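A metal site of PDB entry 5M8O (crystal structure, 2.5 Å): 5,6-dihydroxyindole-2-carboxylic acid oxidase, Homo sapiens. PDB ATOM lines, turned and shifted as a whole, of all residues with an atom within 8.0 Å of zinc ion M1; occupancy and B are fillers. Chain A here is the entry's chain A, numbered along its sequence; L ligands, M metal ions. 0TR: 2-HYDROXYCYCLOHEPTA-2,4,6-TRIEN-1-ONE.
ND1 of His 353 is in hydrogen-bond range of OD1 of Asn 354 (3.1 Å). O of Phe 196 sits at hydrogen-bond distance from ND1 of His 200, at 3.1 Å. O of Glu 336 lies within hydrogen-bond range of ND1 of His 353 (3.1 Å). O of Gly 364 lies within hydrogen-bond range of ND1 of His 357.
NE2 of His 200 touches zinc ion M1, 3.8 Å away. Phe 376 touches zinc ion M1. Within 4 Å of zinc ion M1: His 200, His 353, His 357, Phe 376 and His 380. The nearest printed residue that does not touch zinc ion M1 is Leu 379 (4.5 Å).
Zinc ion M1 is bound by a ring nitrogen (NE2) of His 380, a ring nitrogen (NE2) of His 353 and a ring nitrogen (NE2) of His 357. Zinc ion M1 has three donor atoms within binding distance.
The side-chain hydroxyl (OG) of Ser 370 sits close to an oxygen (OA1) of the ligand, at 3.2 Å. A ring nitrogen (NE2) of His 353 sits close to an oxygen (OA2) of the ligand (3.3 Å).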
ATOM      1  N   HIS A 168     -23.085   8.860 -16.427  1.00  0.00           N
ATOM      2  CA  HIS A 168     -22.898  10.123 -15.714  1.00  0.00           C
ATOM      3  C   HIS A 168     -23.904  10.251 -14.575  1.00  0.00           C
ATOM      4  O   HIS A 168     -23.534  10.602 -13.460  1.00  0.00           O
ATOM      5  CB  HIS A 168     -23.019  11.295 -16.680  1.00  0.00           C
ATOM      6  CG  HIS A 168     -22.696  12.622 -16.082  1.00  0.00           C
ATOM      7  ND1 HIS A 168     -23.656  13.473 -15.588  1.00  0.00           N
ATOM      8  CD2 HIS A 168     -21.515  13.288 -15.957  1.00  0.00           C
ATOM      9  CE1 HIS A 168     -23.087  14.586 -15.152  1.00  0.00           C
ATOM     10  NE2 HIS A 168     -21.788  14.498 -15.371  1.00  0.00           N
ATOM     11  N   SER A 190     -17.679  11.233  -9.935  1.00  0.00           N
ATOM     12  CA  SER A 190     -17.090  11.779 -11.147  1.00  0.00           C
ATOM     13  C   SER A 190     -16.891  13.289 -11.121  1.00  0.00           C
ATOM     14  O   SER A 190     -16.425  13.844 -12.108  1.00  0.00           O
ATOM     15  CB  SER A 190     -17.925  11.404 -12.375  1.00  0.00           C
ATOM     16  OG  SER A 190     -19.288  11.689 -12.156  1.00  0.00           O
ATOM     17  N   HIS A 191     -17.198  13.949 -10.017  1.00  0.00           N
ATOM     18  CA  HIS A 191     -16.975  15.384  -9.880  1.00  0.00           C
ATOM     19  C   HIS A 191     -16.345  15.665  -8.531  1.00  0.00           C
ATOM     20  O   HIS A 191     -16.312  14.812  -7.652  1.00  0.00           O
ATOM     21  CB  HIS A 191     -18.286  16.165 -10.033  1.00  0.00           C
ATOM     22  CG  HIS A 191     -19.043  15.845 -11.281  1.00  0.00           C
ATOM     23  ND1 HIS A 191     -19.608  14.615 -11.519  1.00  0.00           N
ATOM     24  CD2 HIS A 191     -19.297  16.585 -12.384  1.00  0.00           C
ATOM     25  CE1 HIS A 191     -20.182  14.605 -12.697  1.00  0.00           C
ATOM     26  NE2 HIS A 191     -20.016  15.790 -13.244  1.00  0.00           N
ATOM     27  N   PHE A 196     -12.214  13.423 -11.652  1.00  0.00           N
ATOM     28  CA  PHE A 196     -13.055  14.177 -12.573  1.00  0.00           C
ATOM     29  C   PHE A 196     -12.530  14.170 -13.999  1.00  0.00           C
ATOM     30  O   PHE A 196     -13.298  13.948 -14.938  1.00  0.00           O
ATOM     31  CB  PHE A 196     -13.192  15.605 -12.092  1.00  0.00           C
ATOM     32  CG  PHE A 196     -13.639  16.553 -13.132  1.00  0.00           C
ATOM     33  CD1 PHE A 196     -14.945  16.570 -13.548  1.00  0.00           C
ATOM     34  CD2 PHE A 196     -12.748  17.424 -13.712  1.00  0.00           C
ATOM     35  CE1 PHE A 196     -15.347  17.441 -14.514  1.00  0.00           C
ATOM     36  CE2 PHE A 196     -13.159  18.284 -14.673  1.00  0.00           C
ATOM     37  CZ  PHE A 196     -14.462  18.295 -15.076  1.00  0.00           C
ATOM     38  N   TRP A 199     -12.146  10.310 -15.290  1.00  0.00           N
ATOM     39  CA  TRP A 199     -13.499   9.806 -15.497  1.00  0.00           C
ATOM     40  C   TRP A 199     -14.067  10.295 -16.831  1.00  0.00           C
ATOM     41  O   TRP A 199     -14.484   9.511 -17.681  1.00  0.00           O
ATOM     42  CB  TRP A 199     -14.419  10.239 -14.343  1.00  0.00           C
ATOM     43  CG  TRP A 199     -15.714   9.489 -14.319  1.00  0.00           C
ATOM     44  CD1 TRP A 199     -16.010   8.449 -13.521  1.00  0.00           C
ATOM     45  CD2 TRP A 199     -16.849   9.713 -15.138  1.00  0.00           C
ATOM     46  NE1 TRP A 199     -17.252   7.995 -13.788  1.00  0.00           N
ATOM     47  CE2 TRP A 199     -17.795   8.752 -14.788  1.00  0.00           C
ATOM     48  CE3 TRP A 199     -17.170  10.615 -16.152  1.00  0.00           C
ATOM     49  CZ2 TRP A 199     -19.058   8.682 -15.403  1.00  0.00           C
ATOM     50  CZ3 TRP A 199     -18.407  10.541 -16.750  1.00  0.00           C
ATOM     51  CH2 TRP A 199     -19.340   9.579 -16.380  1.00  0.00           C
ATOM     52  N   HIS A 200     -14.049  11.579 -17.027  1.00  0.00           N
ATOM     53  CA  HIS A 200     -14.664  12.136 -18.170  1.00  0.00           C
ATOM     54  C   HIS A 200     -13.895  11.826 -19.436  1.00  0.00           C
ATOM     55  O   HIS A 200     -14.461  11.827 -20.484  1.00  0.00           O
ATOM     56  CB  HIS A 200     -14.929  13.632 -17.982  1.00  0.00           C
ATOM     57  CG  HIS A 200     -16.176  13.968 -17.207  1.00  0.00           C
ATOM     58  ND1 HIS A 200     -16.239  13.902 -15.839  1.00  0.00           N
ATOM     59  CD2 HIS A 200     -17.378  14.427 -17.602  1.00  0.00           C
ATOM     60  CE1 HIS A 200     -17.424  14.286 -15.441  1.00  0.00           C
ATOM     61  NE2 HIS A 200     -18.126  14.614 -16.484  1.00  0.00           N
ATOM     62  N   HIS A 203     -15.188   8.452 -20.346  1.00  0.00           N
ATOM     63  CA  HIS A 203     -16.526   8.743 -20.834  1.00  0.00           C
ATOM     64  C   HIS A 203     -16.541   9.014 -22.320  1.00  0.00           C
ATOM     65  O   HIS A 203     -17.292   8.389 -23.079  1.00  0.00           O
ATOM     66  CB  HIS A 203     -17.083   9.931 -20.053  1.00  0.00           C
ATOM     67  CG  HIS A 203     -18.573  10.029 -20.024  1.00  0.00           C
ATOM     68  ND1 HIS A 203     -19.234  11.229 -19.986  1.00  0.00           N
ATOM     69  CD2 HIS A 203     -19.521   9.073 -19.956  1.00  0.00           C
ATOM     70  CE1 HIS A 203     -20.528  11.019 -19.916  1.00  0.00           C
ATOM     71  NE2 HIS A 203     -20.729   9.710 -19.911  1.00  0.00           N
ATOM     72  N   GLU A 336     -11.723  22.052 -13.677  1.00  0.00           N
ATOM     73  CA  GLU A 336     -13.079  21.657 -13.333  1.00  0.00           C
ATOM     74  C   GLU A 336     -13.929  22.877 -13.052  1.00  0.00           C
ATOM     75  O   GLU A 336     -15.120  22.886 -13.366  1.00  0.00           O
ATOM     76  CB  GLU A 336     -13.088  20.722 -12.121  1.00  0.00           C
ATOM     77  CG  GLU A 336     -14.472  20.199 -11.800  1.00  0.00           C
ATOM     78  CD  GLU A 336     -14.486  19.139 -10.716  1.00  0.00           C
ATOM     79  OE1 GLU A 336     -13.405  18.790 -10.207  1.00  0.00           O
ATOM     80  OE2 GLU A 336     -15.579  18.653 -10.386  1.00  0.00           O
ATOM     81  N   HIS A 353     -14.886  24.743 -16.963  1.00  0.00           N
ATOM     82  CA  HIS A 353     -15.839  23.666 -17.222  1.00  0.00           C
ATOM     83  C   HIS A 353     -17.190  23.905 -16.550  1.00  0.00           C
ATOM     84  O   HIS A 353     -18.241  23.807 -17.187  1.00  0.00           O
ATOM     85  CB  HIS A 353     -15.240  22.339 -16.776  1.00  0.00           C
ATOM     86  CG  HIS A 353     -16.246  21.266 -16.467  1.00  0.00           C
ATOM     87  ND1 HIS A 353     -16.742  21.053 -15.205  1.00  0.00           N
ATOM     88  CD2 HIS A 353     -16.835  20.338 -17.256  1.00  0.00           C
ATOM     89  CE1 HIS A 353     -17.589  20.049 -15.227  1.00  0.00           C
ATOM     90  NE2 HIS A 353     -17.675  19.601 -16.465  1.00  0.00           N
ATOM     91  N   ASN A 354     -17.179  24.203 -15.248  1.00  0.00           N
ATOM     92  CA  ASN A 354     -18.429  24.486 -14.560  1.00  0.00           C
ATOM     93  C   ASN A 354     -19.170  25.659 -15.185  1.00  0.00           C
ATOM     94  O   ASN A 354     -20.391  25.635 -15.344  1.00  0.00           O
ATOM     95  CB  ASN A 354     -18.150  24.752 -13.095  1.00  0.00           C
ATOM     96  CG  ASN A 354     -17.829  23.521 -12.338  1.00  0.00           C
ATOM     97  OD1 ASN A 354     -18.127  22.420 -12.772  1.00  0.00           O
ATOM     98  ND2 ASN A 354     -17.185  23.679 -11.215  1.00  0.00           N
ATOM     99  N   ALA A 356     -19.027  26.764 -18.309  1.00  0.00           N
ATOM    100  CA  ALA A 356     -19.609  26.398 -19.596  1.00  0.00           C
ATOM    101  C   ALA A 356     -20.895  25.608 -19.427  1.00  0.00           C
ATOM    102  O   ALA A 356     -21.824  25.758 -20.208  1.00  0.00           O
ATOM    103  CB  ALA A 356     -18.586  25.608 -20.415  1.00  0.00           C
ATOM    104  N   HIS A 357     -20.970  24.773 -18.384  1.00  0.00           N
ATOM    105  CA  HIS A 357     -22.208  24.064 -18.091  1.00  0.00           C
ATOM    106  C   HIS A 357     -23.316  25.030 -17.721  1.00  0.00           C
ATOM    107  O   HIS A 357     -24.395  25.029 -18.331  1.00  0.00           O
ATOM    108  CB  HIS A 357     -21.999  23.085 -16.949  1.00  0.00           C
ATOM    109  CG  HIS A 357     -21.567  21.713 -17.364  1.00  0.00           C
ATOM    110  ND1 HIS A 357     -22.461  20.737 -17.744  1.00  0.00           N
ATOM    111  CD2 HIS A 357     -20.349  21.142 -17.412  1.00  0.00           C
ATOM    112  CE1 HIS A 357     -21.801  19.629 -18.032  1.00  0.00           C
ATOM    113  NE2 HIS A 357     -20.519  19.850 -17.825  1.00  0.00           N
ATOM    114  N   GLY A 364     -28.325  21.265 -19.790  1.00  0.00           N
ATOM    115  CA  GLY A 364     -26.892  21.140 -19.766  1.00  0.00           C
ATOM    116  C   GLY A 364     -26.232  21.636 -18.496  1.00  0.00           C
ATOM    117  O   GLY A 364     -25.034  21.400 -18.313  1.00  0.00           O
ATOM    118  N   THR A 367     -26.694  18.677 -12.804  1.00  0.00           N
ATOM    119  CA  THR A 367     -25.703  17.627 -12.621  1.00  0.00           C
ATOM    120  C   THR A 367     -26.243  16.247 -12.972  1.00  0.00           C
ATOM    121  O   THR A 367     -25.578  15.476 -13.674  1.00  0.00           O
ATOM    122  CB  THR A 367     -25.175  17.671 -11.196  1.00  0.00           C
ATOM    123  OG1 THR A 367     -24.789  19.015 -10.895  1.00  0.00           O
ATOM    124  CG2 THR A 367     -23.990  16.754 -11.035  1.00  0.00           C
ATOM    125  N   SER A 370     -26.992  16.557 -17.295  1.00  0.00           N
ATOM    126  CA  SER A 370     -26.372  17.404 -18.309  1.00  0.00           C
ATOM    127  C   SER A 370     -25.902  16.716 -19.592  1.00  0.00           C
ATOM    128  O   SER A 370     -25.781  17.394 -20.613  1.00  0.00           O
ATOM    129  CB  SER A 370     -25.225  18.177 -17.691  1.00  0.00           C
ATOM    130  OG  SER A 370     -24.269  17.316 -17.183  1.00  0.00           O
ATOM    131  N   PRO A 371     -25.568  15.426 -19.624  1.00  0.00           N
ATOM    132  CA  PRO A 371     -25.266  14.828 -20.928  1.00  0.00           C
ATOM    133  C   PRO A 371     -26.482  14.706 -21.854  1.00  0.00           C
ATOM    134  O   PRO A 371     -26.292  14.436 -23.038  1.00  0.00           O
ATOM    135  CB  PRO A 371     -24.698  13.453 -20.563  1.00  0.00           C
ATOM    136  CG  PRO A 371     -24.265  13.593 -19.194  1.00  0.00           C
ATOM    137  CD  PRO A 371     -25.171  14.538 -18.531  1.00  0.00           C
ATOM    138  N   PHE A 376     -22.837  18.743 -24.300  1.00  0.00           N
ATOM    139  CA  PHE A 376     -21.982  18.092 -23.310  1.00  0.00           C
ATOM    140  C   PHE A 376     -20.768  17.444 -23.956  1.00  0.00           C
ATOM    141  O   PHE A 376     -19.622  17.677 -23.520  1.00  0.00           O
ATOM    142  CB  PHE A 376     -22.836  17.087 -22.539  1.00  0.00           C
ATOM    143  CG  PHE A 376     -22.122  16.399 -21.445  1.00  0.00           C
ATOM    144  CD1 PHE A 376     -21.311  15.332 -21.695  1.00  0.00           C
ATOM    145  CD2 PHE A 376     -22.275  16.835 -20.150  1.00  0.00           C
ATOM    146  CE1 PHE A 376     -20.682  14.697 -20.670  1.00  0.00           C
ATOM    147  CE2 PHE A 376     -21.635  16.205 -19.117  1.00  0.00           C
ATOM    148  CZ  PHE A 376     -20.840  15.146 -19.376  1.00  0.00           C
ATOM    149  N   LEU A 379     -18.386  20.116 -24.993  1.00  0.00           N
ATOM    150  CA  LEU A 379     -17.864  20.764 -23.807  1.00  0.00           C
ATOM    151  C   LEU A 379     -16.740  19.948 -23.199  1.00  0.00           C
ATOM    152  O   LEU A 379     -15.720  20.487 -22.794  1.00  0.00           O
ATOM    153  CB  LEU A 379     -19.000  20.967 -22.814  1.00  0.00           C
ATOM    154  CG  LEU A 379     -18.787  21.849 -21.602  1.00  0.00           C
ATOM    155  CD1 LEU A 379     -20.128  22.276 -21.067  1.00  0.00           C
ATOM    156  CD2 LEU A 379     -18.017  21.099 -20.532  1.00  0.00           C
ATOM    157  N   HIS A 380     -16.893  18.629 -23.177  1.00  0.00           N
ATOM    158  CA  HIS A 380     -15.940  17.803 -22.454  1.00  0.00           C
ATOM    159  C   HIS A 380     -14.770  17.354 -23.307  1.00  0.00           C
ATOM    160  O   HIS A 380     -13.702  17.079 -22.753  1.00  0.00           O
ATOM    161  CB  HIS A 380     -16.648  16.614 -21.797  1.00  0.00           C
ATOM    162  CG  HIS A 380     -17.089  16.899 -20.399  1.00  0.00           C
ATOM    163  ND1 HIS A 380     -16.237  16.842 -19.329  1.00  0.00           N
ATOM    164  CD2 HIS A 380     -18.282  17.301 -19.904  1.00  0.00           C
ATOM    165  CE1 HIS A 380     -16.882  17.185 -18.229  1.00  0.00           C
ATOM    166  NE2 HIS A 380     -18.130  17.469 -18.547  1.00  0.00           N
ATOM    167  N   THR A 383     -12.592  20.206 -22.636  1.00  0.00           N
ATOM    168  CA  THR A 383     -12.012  20.021 -21.313  1.00  0.00           C
ATOM    169  C   THR A 383     -10.952  18.941 -21.323  1.00  0.00           C
ATOM    170  O   THR A 383      -9.925  19.084 -20.668  1.00  0.00           O
ATOM    171  CB  THR A 383     -13.094  19.671 -20.319  1.00  0.00           C
ATOM    172  OG1 THR A 383     -14.148  20.615 -20.420  1.00  0.00           O
ATOM    173  CG2 THR A 383     -12.539  19.665 -18.899  1.00  0.00           C
HETATM  174  CA1 0TR L   1     -22.283  19.007 -14.491  1.00  0.00           C
HETATM  175  OA1 0TR L   1     -22.045  17.666 -14.847  1.00  0.00           O
HETATM  176  CA2 0TR L   1     -21.140  19.685 -14.155  1.00  0.00           C
HETATM  177  OA2 0TR L   1     -20.053  18.856 -14.276  1.00  0.00           O
HETATM  178  CA3 0TR L   1     -20.930  20.985 -13.738  1.00  0.00           C
HETATM  179  CB3 0TR L   1     -21.873  21.977 -13.569  1.00  0.00           C
HETATM  180  CA5 0TR L   1     -23.978  20.785 -14.168  1.00  0.00           C
HETATM  181  CA6 0TR L   1     -23.569  19.501 -14.506  1.00  0.00           C
HETATM  182  CAE 0TR L   1     -23.229  21.871 -13.764  1.00  0.00           C
HETATM  183 ZN    ZN M   1     -19.105  18.277 -17.151  1.00  0.00          ZN
HETATM  184 ZN    ZN M   2     -20.778  16.449 -15.127  1.00  0.00          ZN
